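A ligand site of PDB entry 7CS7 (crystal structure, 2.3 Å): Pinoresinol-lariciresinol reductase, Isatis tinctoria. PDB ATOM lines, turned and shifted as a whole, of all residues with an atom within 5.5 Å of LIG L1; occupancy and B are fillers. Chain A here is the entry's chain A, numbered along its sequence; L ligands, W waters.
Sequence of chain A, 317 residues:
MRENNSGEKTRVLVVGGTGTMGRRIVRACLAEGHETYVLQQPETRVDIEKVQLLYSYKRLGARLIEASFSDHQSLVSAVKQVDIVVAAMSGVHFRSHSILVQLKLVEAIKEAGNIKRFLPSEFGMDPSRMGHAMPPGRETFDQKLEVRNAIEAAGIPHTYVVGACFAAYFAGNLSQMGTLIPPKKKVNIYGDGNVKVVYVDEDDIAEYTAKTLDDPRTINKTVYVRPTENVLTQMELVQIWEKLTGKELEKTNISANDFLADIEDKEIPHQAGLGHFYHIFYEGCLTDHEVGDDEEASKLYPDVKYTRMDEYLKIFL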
ATOM      1  N   VAL A  15     -12.209 -20.272 -27.280  1.00  0.00           N
ATOM      2  CA  VAL A  15     -10.929 -19.808 -27.787  1.00  0.00           C
ATOM      3  C   VAL A  15     -10.877 -18.309 -27.569  1.00  0.00           C
ATOM      4  O   VAL A  15     -11.830 -17.601 -27.877  1.00  0.00           O
ATOM      5  CB  VAL A  15     -10.768 -20.178 -29.266  1.00  0.00           C
ATOM      6  CG1 VAL A  15      -9.467 -19.636 -29.846  1.00  0.00           C
ATOM      7  CG2 VAL A  15     -10.850 -21.704 -29.407  1.00  0.00           C
ATOM      8  N   GLY A  16      -9.773 -17.843 -27.002  1.00  0.00           N
ATOM      9  CA  GLY A  16      -9.690 -16.472 -26.547  1.00  0.00           C
ATOM     10  C   GLY A  16     -10.329 -16.241 -25.206  1.00  0.00           C
ATOM     11  O   GLY A  16     -10.896 -15.165 -24.965  1.00  0.00           O
ATOM     12  N   GLY A  17     -10.251 -17.222 -24.313  1.00  0.00           N
ATOM     13  CA  GLY A  17     -10.947 -17.161 -23.047  1.00  0.00           C
ATOM     14  C   GLY A  17     -10.366 -16.240 -21.990  1.00  0.00           C
ATOM     15  O   GLY A  17     -10.985 -16.079 -20.934  1.00  0.00           O
ATOM     16  N   THR A  18      -9.202 -15.639 -22.204  1.00  0.00           N
ATOM     17  CA  THR A  18      -8.721 -14.605 -21.288  1.00  0.00           C
ATOM     18  C   THR A  18      -9.012 -13.192 -21.784  1.00  0.00           C
ATOM     19  O   THR A  18      -8.557 -12.230 -21.156  1.00  0.00           O
ATOM     20  CB  THR A  18      -7.216 -14.741 -21.044  1.00  0.00           C
ATOM     21  OG1 THR A  18      -6.495 -14.395 -22.218  1.00  0.00           O
ATOM     22  CG2 THR A  18      -6.884 -16.144 -20.612  1.00  0.00           C
ATOM     23  N   GLY A  19      -9.771 -13.043 -22.872  1.00  0.00           N
ATOM     24  CA  GLY A  19     -10.132 -11.734 -23.368  1.00  0.00           C
ATOM     25  C   GLY A  19     -11.315 -11.142 -22.641  1.00  0.00           C
ATOM     26  O   GLY A  19     -11.977 -11.795 -21.836  1.00  0.00           O
ATOM     27  N   THR A  20     -11.553  -9.859 -22.930  1.00  0.00           N
ATOM     28  CA  THR A  20     -12.667  -9.135 -22.349  1.00  0.00           C
ATOM     29  C   THR A  20     -13.968  -9.909 -22.505  1.00  0.00           C
ATOM     30  O   THR A  20     -14.749 -10.056 -21.554  1.00  0.00           O
ATOM     31  CB  THR A  20     -12.825  -7.771 -23.005  1.00  0.00           C
ATOM     32  OG1 THR A  20     -11.629  -7.010 -22.826  1.00  0.00           O
ATOM     33  CG2 THR A  20     -14.024  -7.028 -22.420  1.00  0.00           C
ATOM     34  N   MET A  21     -14.246 -10.346 -23.730  1.00  0.00           N
ATOM     35  CA  MET A  21     -15.470 -11.060 -24.028  1.00  0.00           C
ATOM     36  C   MET A  21     -15.314 -12.560 -23.819  1.00  0.00           C
ATOM     37  O   MET A  21     -16.265 -13.218 -23.384  1.00  0.00           O
ATOM     38  CB  MET A  21     -15.895 -10.766 -25.476  1.00  0.00           C
ATOM     39  CG  MET A  21     -17.247 -11.354 -25.866  1.00  0.00           C
ATOM     40  SD  MET A  21     -18.625 -10.420 -25.205  1.00  0.00           S
ATOM     41  CE  MET A  21     -19.373 -11.628 -24.154  1.00  0.00           C
ATOM     42  N   GLY A  22     -14.110 -13.097 -24.056  1.00  0.00           N
ATOM     43  CA  GLY A  22     -13.886 -14.512 -23.864  1.00  0.00           C
ATOM     44  C   GLY A  22     -14.094 -14.960 -22.433  1.00  0.00           C
ATOM     45  O   GLY A  22     -14.744 -15.980 -22.190  1.00  0.00           O
ATOM     46  N   LEU A  39      -9.031 -23.012 -24.301  1.00  0.00           N
ATOM     47  CA  LEU A  39      -7.753 -23.159 -24.966  1.00  0.00           C
ATOM     48  C   LEU A  39      -6.676 -22.387 -24.218  1.00  0.00           C
ATOM     49  O   LEU A  39      -6.807 -21.176 -23.985  1.00  0.00           O
ATOM     50  CB  LEU A  39      -7.832 -22.664 -26.404  1.00  0.00           C
ATOM     51  CG  LEU A  39      -6.638 -23.137 -27.223  1.00  0.00           C
ATOM     52  CD1 LEU A  39      -6.926 -24.530 -27.761  1.00  0.00           C
ATOM     53  CD2 LEU A  39      -6.328 -22.185 -28.344  1.00  0.00           C
ATOM     54  N   GLN A  41      -3.008 -21.163 -24.496  1.00  0.00           N
ATOM     55  CA  GLN A  41      -1.927 -20.940 -25.446  1.00  0.00           C
ATOM     56  C   GLN A  41      -0.595 -20.769 -24.725  1.00  0.00           C
ATOM     57  O   GLN A  41      -0.558 -20.286 -23.591  1.00  0.00           O
ATOM     58  CB  GLN A  41      -2.210 -19.699 -26.279  1.00  0.00           C
ATOM     59  CG  GLN A  41      -3.448 -19.806 -27.129  1.00  0.00           C
ATOM     60  CD  GLN A  41      -3.647 -18.603 -28.020  1.00  0.00           C
ATOM     61  OE1 GLN A  41      -4.628 -17.871 -27.887  1.00  0.00           O
ATOM     62  NE2 GLN A  41      -2.704 -18.372 -28.930  1.00  0.00           N
ATOM     63  N   GLU A  43       1.510 -18.674 -24.412  1.00  0.00           N
ATOM     64  CA  GLU A  43       1.483 -17.356 -23.763  1.00  0.00           C
ATOM     65  C   GLU A  43       1.610 -17.325 -22.222  1.00  0.00           C
ATOM     66  O   GLU A  43       0.812 -16.676 -21.536  1.00  0.00           O
ATOM     67  CB  GLU A  43       0.185 -16.675 -24.267  1.00  0.00           C
ATOM     68  CG  GLU A  43      -0.869 -16.107 -23.275  1.00  0.00           C
ATOM     69  CD  GLU A  43      -1.682 -17.181 -22.522  1.00  0.00           C
ATOM     70  OE1 GLU A  43      -1.649 -17.205 -21.267  1.00  0.00           O
ATOM     71  OE2 GLU A  43      -2.368 -18.002 -23.176  1.00  0.00           O
ATOM     72  N   LYS A  50      -3.197 -13.290 -17.351  1.00  0.00           N
ATOM     73  CA  LYS A  50      -3.716 -14.414 -18.123  1.00  0.00           C
ATOM     74  C   LYS A  50      -3.657 -15.713 -17.329  1.00  0.00           C
ATOM     75  O   LYS A  50      -4.651 -16.446 -17.233  1.00  0.00           O
ATOM     76  CB  LYS A  50      -2.966 -14.539 -19.443  1.00  0.00           C
ATOM     77  CG  LYS A  50      -3.345 -13.508 -20.472  1.00  0.00           C
ATOM     78  CD  LYS A  50      -2.649 -13.780 -21.800  1.00  0.00           C
ATOM     79  CE  LYS A  50      -2.834 -12.614 -22.761  1.00  0.00           C
ATOM     80  NZ  LYS A  50      -4.279 -12.257 -22.895  1.00  0.00           N
ATOM     81  N   PHE A  69      -1.687 -21.952 -32.001  1.00  0.00           N
ATOM     82  CA  PHE A  69      -2.186 -21.663 -33.332  1.00  0.00           C
ATOM     83  C   PHE A  69      -1.159 -21.958 -34.416  1.00  0.00           C
ATOM     84  O   PHE A  69      -1.548 -22.119 -35.582  1.00  0.00           O
ATOM     85  CB  PHE A  69      -2.632 -20.212 -33.417  1.00  0.00           C
ATOM     86  CG  PHE A  69      -3.951 -19.967 -32.763  1.00  0.00           C
ATOM     87  CD1 PHE A  69      -5.092 -20.478 -33.313  1.00  0.00           C
ATOM     88  CD2 PHE A  69      -4.022 -19.246 -31.594  1.00  0.00           C
ATOM     89  CE1 PHE A  69      -6.302 -20.249 -32.716  1.00  0.00           C
ATOM     90  CE2 PHE A  69      -5.227 -19.019 -30.989  1.00  0.00           C
ATOM     91  CZ  PHE A  69      -6.373 -19.528 -31.547  1.00  0.00           C
ATOM     92  N   ALA A  88     -13.526 -15.794 -29.449  1.00  0.00           N
ATOM     93  CA  ALA A  88     -13.708 -14.373 -29.166  1.00  0.00           C
ATOM     94  C   ALA A  88     -12.324 -13.740 -29.129  1.00  0.00           C
ATOM     95  O   ALA A  88     -11.770 -13.498 -28.064  1.00  0.00           O
ATOM     96  CB  ALA A  88     -14.476 -14.148 -27.872  1.00  0.00           C
ATOM     97  N   MET A  89     -11.782 -13.477 -30.306  1.00  0.00           N
ATOM     98  CA  MET A  89     -10.447 -12.932 -30.507  1.00  0.00           C
ATOM     99  C   MET A  89     -10.447 -11.411 -30.384  1.00  0.00           C
ATOM    100  O   MET A  89     -11.487 -10.754 -30.477  1.00  0.00           O
ATOM    101  CB  MET A  89      -9.938 -13.303 -31.900  1.00  0.00           C
ATOM    102  CG  MET A  89     -10.243 -14.728 -32.307  1.00  0.00           C
ATOM    103  SD  MET A  89      -9.365 -15.830 -31.218  1.00  0.00           S
ATOM    104  CE  MET A  89      -7.708 -15.145 -31.268  1.00  0.00           C
ATOM    105  N   SER A  90      -9.262 -10.835 -30.216  1.00  0.00           N
ATOM    106  CA  SER A  90      -9.102  -9.391 -30.379  1.00  0.00           C
ATOM    107  C   SER A  90      -9.690  -8.936 -31.719  1.00  0.00           C
ATOM    108  O   SER A  90      -9.462  -9.562 -32.754  1.00  0.00           O
ATOM    109  CB  SER A  90      -7.628  -9.018 -30.293  1.00  0.00           C
ATOM    110  OG  SER A  90      -7.346  -7.836 -31.036  1.00  0.00           O
ATOM    111  N   GLY A  91     -10.456  -7.851 -31.684  1.00  0.00           N
ATOM    112  CA  GLY A  91     -11.152  -7.388 -32.881  1.00  0.00           C
ATOM    113  C   GLY A  91     -11.243  -5.885 -33.011  1.00  0.00           C
ATOM    114  O   GLY A  91     -10.241  -5.179 -32.867  1.00  0.00           O
ATOM    115  N   HIS A  97      -2.471 -11.424 -37.035  1.00  0.00           N
ATOM    116  CA  HIS A  97      -3.573 -10.530 -36.699  1.00  0.00           C
ATOM    117  C   HIS A  97      -4.885 -11.309 -36.419  1.00  0.00           C
ATOM    118  O   HIS A  97      -5.385 -12.068 -37.257  1.00  0.00           O
ATOM    119  CB  HIS A  97      -3.802  -9.491 -37.809  1.00  0.00           C
ATOM    120  CG  HIS A  97      -4.621  -8.318 -37.361  1.00  0.00           C
ATOM    121  ND1 HIS A  97      -4.217  -7.447 -36.364  1.00  0.00           N
ATOM    122  CD2 HIS A  97      -5.839  -7.872 -37.766  1.00  0.00           C
ATOM    123  CE1 HIS A  97      -5.134  -6.520 -36.180  1.00  0.00           C
ATOM    124  NE2 HIS A  97      -6.130  -6.758 -37.023  1.00  0.00           N
ATOM    125  N   SER A  98      -5.460 -11.020 -35.250  1.00  0.00           N
ATOM    126  CA  SER A  98      -6.165 -12.026 -34.472  1.00  0.00           C
ATOM    127  C   SER A  98      -7.398 -12.586 -35.182  1.00  0.00           C
ATOM    128  O   SER A  98      -7.616 -13.795 -35.172  1.00  0.00           O
ATOM    129  CB  SER A  98      -6.536 -11.441 -33.104  1.00  0.00           C
ATOM    130  OG  SER A  98      -7.228 -10.226 -33.281  1.00  0.00           O
ATOM    131  N   ILE A  99      -8.243 -11.735 -35.774  1.00  0.00           N
ATOM    132  CA  ILE A  99      -9.443 -12.255 -36.409  1.00  0.00           C
ATOM    133  C   ILE A  99      -9.097 -13.358 -37.404  1.00  0.00           C
ATOM    134  O   ILE A  99      -9.689 -14.439 -37.381  1.00  0.00           O
ATOM    135  CB  ILE A  99     -10.239 -11.124 -37.084  1.00  0.00           C
ATOM    136  CG1 ILE A  99     -10.767 -10.168 -36.018  1.00  0.00           C
ATOM    137  CG2 ILE A  99     -11.416 -11.698 -37.888  1.00  0.00           C
ATOM    138  CD1 ILE A  99     -11.893 -10.762 -35.187  1.00  0.00           C
ATOM    139  N   VAL A 101      -6.597 -15.266 -37.514  1.00  0.00           N
ATOM    140  CA  VAL A 101      -6.083 -16.461 -36.838  1.00  0.00           C
ATOM    141  C   VAL A 101      -7.127 -17.568 -36.806  1.00  0.00           C
ATOM    142  O   VAL A 101      -6.788 -18.752 -36.756  1.00  0.00           O
ATOM    143  CB  VAL A 101      -5.603 -16.094 -35.424  1.00  0.00           C
ATOM    144  CG1 VAL A 101      -5.686 -17.281 -34.499  1.00  0.00           C
ATOM    145  CG2 VAL A 101      -4.191 -15.555 -35.468  1.00  0.00           C
ATOM    146  N   SER A 121     -15.699 -15.179 -33.969  1.00  0.00           N
ATOM    147  CA  SER A 121     -15.567 -13.960 -33.194  1.00  0.00           C
ATOM    148  C   SER A 121     -16.313 -12.845 -33.910  1.00  0.00           C
ATOM    149  O   SER A 121     -15.756 -12.186 -34.789  1.00  0.00           O
ATOM    150  CB  SER A 121     -14.110 -13.600 -32.999  1.00  0.00           C
ATOM    151  OG  SER A 121     -14.011 -12.573 -32.045  1.00  0.00           O
ATOM    152  N   GLU A 122     -17.561 -12.618 -33.513  1.00  0.00           N
ATOM    153  CA  GLU A 122     -18.385 -11.590 -34.129  1.00  0.00           C
ATOM    154  C   GLU A 122     -18.729 -10.559 -33.065  1.00  0.00           C
ATOM    155  O   GLU A 122     -17.912  -9.683 -32.771  1.00  0.00           O
ATOM    156  CB  GLU A 122     -19.616 -12.237 -34.772  1.00  0.00           C
ATOM    157  CG  GLU A 122     -19.257 -13.207 -35.858  1.00  0.00           C
ATOM    158  CD  GLU A 122     -19.408 -12.575 -37.235  1.00  0.00           C
ATOM    159  OE1 GLU A 122     -18.747 -13.033 -38.192  1.00  0.00           O
ATOM    160  OE2 GLU A 122     -20.177 -11.612 -37.352  1.00  0.00           O
ATOM    161  N   PHE A 123     -19.927 -10.612 -32.469  1.00  0.00           N
ATOM    162  CA  PHE A 123     -20.309  -9.765 -31.333  1.00  0.00           C
ATOM    163  C   PHE A 123     -20.166  -8.278 -31.637  1.00  0.00           C
ATOM    164  O   PHE A 123     -19.541  -7.531 -30.881  1.00  0.00           O
ATOM    165  CB  PHE A 123     -19.507 -10.107 -30.083  1.00  0.00           C
ATOM    166  CG  PHE A 123     -19.331 -11.553 -29.864  1.00  0.00           C
ATOM    167  CD1 PHE A 123     -18.087 -12.136 -29.989  1.00  0.00           C
ATOM    168  CD2 PHE A 123     -20.430 -12.355 -29.568  1.00  0.00           C
ATOM    169  CE1 PHE A 123     -17.935 -13.494 -29.806  1.00  0.00           C
ATOM    170  CE2 PHE A 123     -20.284 -13.707 -29.380  1.00  0.00           C
ATOM    171  CZ  PHE A 123     -19.028 -14.279 -29.487  1.00  0.00           C
ATOM    172  N   GLY A 124     -20.769  -7.836 -32.718  1.00  0.00           N
ATOM    173  CA  GLY A 124     -20.655  -6.443 -33.086  1.00  0.00           C
ATOM    174  C   GLY A 124     -21.387  -6.185 -34.369  1.00  0.00           C
ATOM    175  O   GLY A 124     -22.290  -6.934 -34.734  1.00  0.00           O
ATOM    176  N   MET A 125     -21.000  -5.108 -35.050  1.00  0.00           N
ATOM    177  CA  MET A 125     -21.585  -4.790 -36.350  1.00  0.00           C
ATOM    178  C   MET A 125     -21.625  -6.025 -37.220  1.00  0.00           C
ATOM    179  O   MET A 125     -20.645  -6.775 -37.295  1.00  0.00           O
ATOM    180  CB  MET A 125     -20.781  -3.699 -37.042  1.00  0.00           C
ATOM    181  CG  MET A 125     -21.236  -2.306 -36.718  1.00  0.00           C
ATOM    182  SD  MET A 125     -20.061  -1.102 -37.326  1.00  0.00           S
ATOM    183  CE  MET A 125     -18.622  -1.559 -36.379  1.00  0.00           C
ATOM    184  N   LYS A 144     -13.655 -10.458 -40.901  1.00  0.00           N
ATOM    185  CA  LYS A 144     -14.714 -11.319 -40.384  1.00  0.00           C
ATOM    186  C   LYS A 144     -15.414 -12.074 -41.516  1.00  0.00           C
ATOM    187  O   LYS A 144     -15.670 -13.275 -41.388  1.00  0.00           O
ATOM    188  CB  LYS A 144     -15.698 -10.506 -39.561  1.00  0.00           C
ATOM    189  CG  LYS A 144     -15.141 -10.198 -38.167  1.00  0.00           C
ATOM    190  CD  LYS A 144     -16.110  -9.427 -37.314  1.00  0.00           C
ATOM    191  CE  LYS A 144     -15.480  -9.044 -35.993  1.00  0.00           C
ATOM    192  NZ  LYS A 144     -16.479  -8.418 -35.090  1.00  0.00           N
ATOM    193  N   ALA A 164     -24.723  -5.647 -31.468  1.00  0.00           N
ATOM    194  CA  ALA A 164     -24.672  -4.938 -30.202  1.00  0.00           C
ATOM    195  C   ALA A 164     -23.468  -4.006 -30.126  1.00  0.00           C
ATOM    196  O   ALA A 164     -22.404  -4.285 -30.679  1.00  0.00           O
ATOM    197  CB  ALA A 164     -24.613  -5.921 -29.030  1.00  0.00           C
ATOM    198  N   CYS A 165     -23.668  -2.894 -29.438  1.00  0.00           N
ATOM    199  CA  CYS A 165     -22.606  -2.042 -28.912  1.00  0.00           C
ATOM    200  C   CYS A 165     -22.265  -2.482 -27.502  1.00  0.00           C
ATOM    201  O   CYS A 165     -23.146  -2.526 -26.643  1.00  0.00           O
ATOM    202  CB  CYS A 165     -23.086  -0.595 -28.861  1.00  0.00           C
ATOM    203  SG  CYS A 165     -22.409   0.420 -30.045  1.00  0.00           S
ATOM    204  N   PHE A 166     -20.990  -2.802 -27.248  1.00  0.00           N
ATOM    205  CA  PHE A 166     -20.587  -3.168 -25.902  1.00  0.00           C
ATOM    206  C   PHE A 166     -20.781  -2.007 -24.954  1.00  0.00           C
ATOM    207  O   PHE A 166     -20.277  -0.906 -25.198  1.00  0.00           O
ATOM    208  CB  PHE A 166     -19.125  -3.611 -25.851  1.00  0.00           C
ATOM    209  CG  PHE A 166     -18.910  -5.009 -26.367  1.00  0.00           C
ATOM    210  CD1 PHE A 166     -19.857  -5.612 -27.168  1.00  0.00           C
ATOM    211  CD2 PHE A 166     -17.765  -5.719 -26.034  1.00  0.00           C
ATOM    212  CE1 PHE A 166     -19.657  -6.878 -27.654  1.00  0.00           C
ATOM    213  CE2 PHE A 166     -17.554  -6.993 -26.517  1.00  0.00           C
ATOM    214  CZ  PHE A 166     -18.512  -7.579 -27.332  1.00  0.00           C
ATOM    215  N   TYR A 169     -17.602  -0.056 -23.782  1.00  0.00           N
ATOM    216  CA  TYR A 169     -16.935   0.826 -24.727  1.00  0.00           C
ATOM    217  C   TYR A 169     -17.815   1.952 -25.240  1.00  0.00           C
ATOM    218  O   TYR A 169     -17.304   2.871 -25.885  1.00  0.00           O
ATOM    219  CB  TYR A 169     -16.406   0.029 -25.907  1.00  0.00           C
ATOM    220  CG  TYR A 169     -15.204  -0.798 -25.544  1.00  0.00           C
ATOM    221  CD1 TYR A 169     -13.970  -0.205 -25.331  1.00  0.00           C
ATOM    222  CD2 TYR A 169     -15.302  -2.177 -25.398  1.00  0.00           C
ATOM    223  CE1 TYR A 169     -12.868  -0.952 -24.977  1.00  0.00           C
ATOM    224  CE2 TYR A 169     -14.201  -2.934 -25.070  1.00  0.00           C
ATOM    225  CZ  TYR A 169     -12.990  -2.320 -24.849  1.00  0.00           C
ATOM    226  OH  TYR A 169     -11.894  -3.079 -24.506  1.00  0.00           O
ATOM    227  N   PHE A 170     -19.115   1.922 -24.993  1.00  0.00           N
ATOM    228  CA  PHE A 170     -20.011   2.903 -25.605  1.00  0.00           C
ATOM    229  C   PHE A 170     -21.054   3.459 -24.662  1.00  0.00           C
ATOM    230  O   PHE A 170     -21.521   4.576 -24.887  1.00  0.00           O
ATOM    231  CB  PHE A 170     -20.725   2.318 -26.825  1.00  0.00           C
ATOM    232  CG  PHE A 170     -19.806   1.963 -27.945  1.00  0.00           C
ATOM    233  CD1 PHE A 170     -19.353   2.943 -28.811  1.00  0.00           C
ATOM    234  CD2 PHE A 170     -19.372   0.672 -28.115  1.00  0.00           C
ATOM    235  CE1 PHE A 170     -18.511   2.633 -29.839  1.00  0.00           C
ATOM    236  CE2 PHE A 170     -18.513   0.361 -29.144  1.00  0.00           C
ATOM    237  CZ  PHE A 170     -18.071   1.340 -30.002  1.00  0.00           C
HETATM  238  P1  LIG L   1      -9.477  -9.217 -26.837  1.00  0.00           P
HETATM  239  O1  LIG L   1      -8.571  -8.037 -27.166  1.00  0.00           O
HETATM  240  O2  LIG L   1      -9.978  -9.113 -25.413  1.00  0.00           O
HETATM  241  O3  LIG L   1      -8.634 -10.624 -27.057  1.00  0.00           O
HETATM  242  C1  LIG L   1      -9.325 -11.800 -26.669  1.00  0.00           C
HETATM  243  C2  LIG L   1      -8.468 -13.032 -27.008  1.00  0.00           C
HETATM  244  O4  LIG L   1      -8.033 -12.927 -28.233  1.00  0.00           O
HETATM  245  C3  LIG L   1      -7.186 -13.062 -26.173  1.00  0.00           C
HETATM  246  O5  LIG L   1      -7.431 -13.512 -24.904  1.00  0.00           O
HETATM  247  C4  LIG L   1      -6.309 -14.024 -27.017  1.00  0.00           C
HETATM  248  O6  LIG L   1      -6.581 -15.454 -26.668  1.00  0.00           O
HETATM  249  C5  LIG L   1      -6.671 -13.793 -28.273  1.00  0.00           C
HETATM  250  N1  LIG L   1      -5.745 -12.963 -29.028  1.00  0.00           N
HETATM  251  C6  LIG L   1      -5.529 -11.655 -29.214  1.00  0.00           C
HETATM  252  N2  LIG L   1      -4.480 -11.516 -30.059  1.00  0.00           N
HETATM  253  C7  LIG L   1      -4.075 -12.755 -30.410  1.00  0.00           C
HETATM  254  C8  LIG L   1      -3.063 -13.178 -31.249  1.00  0.00           C
HETATM  255  N3  LIG L   1      -2.054 -12.507 -32.065  1.00  0.00           N
HETATM  256  N4  LIG L   1      -2.837 -14.466 -31.443  1.00  0.00           N
HETATM  257  C9  LIG L   1      -3.620 -15.376 -30.800  1.00  0.00           C
HETATM  258  N5  LIG L   1      -4.621 -14.976 -29.962  1.00  0.00           N
HETATM  259  C10 LIG L   1      -4.857 -13.656 -29.778  1.00  0.00           C
HETATM  260  O7  LIG L   1     -10.771  -9.232 -27.889  1.00  0.00           O
HETATM  261  P2  LIG L   1     -12.233  -8.464 -27.610  1.00  0.00           P
HETATM  262  O8  LIG L   1     -12.891  -8.957 -26.328  1.00  0.00           O
HETATM  263  O9  LIG L   1     -12.026  -6.960 -27.541  1.00  0.00           O
HETATM  264  O10 LIG L   1     -13.221  -8.847 -28.897  1.00  0.00           O
HETATM  265  C11 LIG L   1     -13.825 -10.122 -28.987  1.00  0.00           C
HETATM  266  C12 LIG L   1     -14.904  -9.995 -30.124  1.00  0.00           C
HETATM  267  O11 LIG L   1     -15.761  -9.091 -29.724  1.00  0.00           O
HETATM  268  C13 LIG L   1     -14.314  -9.460 -31.448  1.00  0.00           C
HETATM  269  O12 LIG L   1     -14.933 -10.030 -32.518  1.00  0.00           O
HETATM  270  C14 LIG L   1     -14.551  -7.928 -31.388  1.00  0.00           C
HETATM  271  O13 LIG L   1     -14.639  -7.307 -32.764  1.00  0.00           O
HETATM  272  C15 LIG L   1     -15.699  -7.833 -30.755  1.00  0.00           C
HETATM  273  N6  LIG L   1     -15.879  -6.582 -30.011  1.00  0.00           N
HETATM  274  C16 LIG L   1     -17.177  -6.019 -29.951  1.00  0.00           C
HETATM  275  C17 LIG L   1     -17.477  -4.757 -29.192  1.00  0.00           C
HETATM  276  C18 LIG L   1     -18.830  -4.059 -29.476  1.00  0.00           C
HETATM  277  O14 LIG L   1     -19.703  -4.653 -30.014  1.00  0.00           O
HETATM  278  N7  LIG L   1     -19.048  -2.697 -29.030  1.00  0.00           N
HETATM  279  C19 LIG L   1     -16.381  -3.968 -28.428  1.00  0.00           C
HETATM  280  C20 LIG L   1     -14.951  -4.457 -28.832  1.00  0.00           C
HETATM  281  C21 LIG L   1     -14.791  -5.922 -29.323  1.00  0.00           C
HETATM  282  P3  LIG L   1      -6.231 -16.076 -25.181  1.00  0.00           P
HETATM  283  O15 LIG L   1      -7.250 -15.614 -24.176  1.00  0.00           O
HETATM  284  O16 LIG L   1      -6.282 -17.585 -25.239  1.00  0.00           O
HETATM  285  O17 LIG L   1      -4.851 -15.583 -24.797  1.00  0.00           O
HETATM  286  C1  LG2 L   2     -14.466   1.836 -30.193  1.00  0.00           C
HETATM  287  C2  LG2 L   2     -16.034  -2.602 -31.898  1.00  0.00           C
HETATM  288  C3  LG2 L   2     -17.393  -2.401 -31.892  1.00  0.00           C
HETATM  289  C4  LG2 L   2     -15.469  -3.429 -32.860  1.00  0.00           C
HETATM  290  C5  LG2 L   2     -12.541   4.148 -27.870  1.00  0.00           C
HETATM  291  C6  LG2 L   2     -16.274  -4.032 -33.816  1.00  0.00           C
HETATM  292  C7  LG2 L   2     -14.763   3.909 -26.974  1.00  0.00           C
HETATM  293  C8  LG2 L   2     -13.476   4.451 -26.888  1.00  0.00           C
HETATM  294  C9  LG2 L   2     -10.260   4.613 -28.754  1.00  0.00           C
HETATM  295  O1  LG2 L   2     -12.865  -1.445 -32.017  1.00  0.00           O
HETATM  296  O2  LG2 L   2     -12.820  -1.429 -29.235  1.00  0.00           O
HETATM  297  O3  LG2 L   2     -19.610  -2.827 -32.847  1.00  0.00           O
HETATM  298  O4  LG2 L   2     -11.252   4.714 -27.754  1.00  0.00           O
HETATM  299  O5  LG2 L   2     -18.465  -4.415 -34.742  1.00  0.00           O
HETATM  300  O6  LG2 L   2     -13.171   5.294 -25.826  1.00  0.00           O
HETATM  301  C10 LG2 L   2     -14.880  -0.458 -31.144  1.00  0.00           C
HETATM  302  C11 LG2 L   2     -14.379   0.321 -29.887  1.00  0.00           C
HETATM  303  C12 LG2 L   2     -15.211  -1.907 -30.795  1.00  0.00           C
HETATM  304  C13 LG2 L   2     -13.861  -0.473 -32.294  1.00  0.00           C
HETATM  305  C14 LG2 L   2     -12.943  -0.043 -29.496  1.00  0.00           C
HETATM  306  C15 LG2 L   2     -14.150   2.746 -28.997  1.00  0.00           C
HETATM  307  C16 LG2 L   2     -12.886   3.305 -28.916  1.00  0.00           C
HETATM  308  C17 LG2 L   2     -15.096   3.067 -28.029  1.00  0.00           C
HETATM  309  C18 LG2 L   2     -18.215  -3.008 -32.824  1.00  0.00           C
HETATM  310  C19 LG2 L   2     -17.643  -3.817 -33.799  1.00  0.00           C
HETATM  311  C20 LG2 L   2     -20.266  -2.070 -31.874  1.00  0.00           C
HETATM  312  O   HOH W   1     -12.244 -12.078 -25.805  1.00  0.00           O
HETATM  313  O   HOH W   2      -1.225 -15.803 -28.564  1.00  0.00           O
HETATM  314  O   HOH W   3      -8.392 -19.113 -24.833  1.00  0.00           O
HETATM  315  O   HOH W   4      -2.570 -14.822 -26.052  1.00  0.00           O
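Water W3 lies within hydrogen-bond range of an oxygen (O16) of LIG L1 (2.6 Å), the backbone NH (N) of Gly 17 (2.7 Å), the backbone carbonyl oxygen (O) of Leu 39 (2.7 Å) and the backbone NH (N) of Gly 16 (2.9 Å).
Water W1 lies within hydrogen-bond range of O of Ala 88 (2.7 Å), N of Gly 22 (2.8 Å), O8 of LIG L1 (3.2 Å), N of Met 21 (3.4 Å) and O of Gly 16 (3.5 Å).
NZ of Lys 50 is in hydrogen-bond range of OG1 of Thr 18 (3.2 Å).
The backbone NH of Met 89 lies within hydrogen-bond range of the side-chain hydroxyl of Ser 121, at 3.0 Å.
The side-chain hydroxyl (OG) of Ser 90 lies close to the side-chain hydroxyl (OG) of Ser 98, 3.3 Å away.
O of Glu 122 is in hydrogen-bond range of NZ of Lys 144 (3.0 Å).
The side-chain carboxylate (OE2) of Glu 43 is in hydrogen-bond range of the backbone NH (N) of Gln 41 (3.5 Å).
N of Ala 88 is in hydrogen-bond range of O of Val 15 (2.9 Å).
N of Thr 18 sits at hydrogen-bond distance from O15 of LIG L1, 2.8 Å away.
OG1 of Thr 18 sits at hydrogen-bond distance from O15 of LIG L1, at 2.4 Å.
N of Phe 166 sits close to N7 of LIG L1 (2.6 Å).
O of Ser 121 sits at hydrogen-bond distance from O12 of LIG L1, 3.2 Å away.
OG of Ser 121 sits at hydrogen-bond distance from O12 of LIG L1 (2.7 Å).
O4 of LIG L1 lies within hydrogen-bond range of N of Ser 90.
The backbone carbonyl oxygen (O) of Glu 122 is in hydrogen-bond range of an oxygen (O12) of LIG L1 (3.0 Å).
N of Thr 20 sits at hydrogen-bond distance from O2 of LIG L1, 3.0 Å away.
The backbone NH of Gly 19 lies within hydrogen-bond range of an oxygen (O5) of LIG L1, 3.1 Å away.
The side-chain amide oxygen of Gln 41 sits close to an oxygen (O16) of LIG L1, 3.1 Å away.
The side-chain amino group (NZ) of Lys 144 is in hydrogen-bond range of an oxygen (O13) of LIG L1, 3.2 Å away.
The backbone NH of Met 21 lies within hydrogen-bond range of an oxygen (O8) of LIG L1, 3.2 Å away.
O15 of LIG L1 lies within hydrogen-bond range of N of Gly 17, at 3.4 Å.
NZ of Lys 50 lies within salt-bridge range of O17 of LIG L1 (3.9 Å).
O5 of LG2 L2 sits at hydrogen-bond distance from N of Met 125.
The backbone carbonyl oxygen (O) of Met 89 sits close to an oxygen (O10) of LIG L1 (3.0 Å).
The backbone carbonyl oxygen (O) of Phe 123 lies close to an oxygen (O14) of LIG L1 (3.0 Å).
An oxygen (O14) of LIG L1 lies close to the backbone carbonyl oxygen (O) of Ala 164 (2.8 Å).
Residues that only touch LIG L1: Gly 16 (3.3 Å), Leu 39 (3.8 Å), Glu 43 (3.8 Å), Phe 69 (3.97 Å), Ala 88 (3.3 Å), Gly 91 (3.5 Å), Ser 98 (3.7 Å), Gly 124 (3.7 Å), Cys 165 (3.6 Å), Tyr 169 (3.7 Å) and Phe 170 (3.1 Å).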
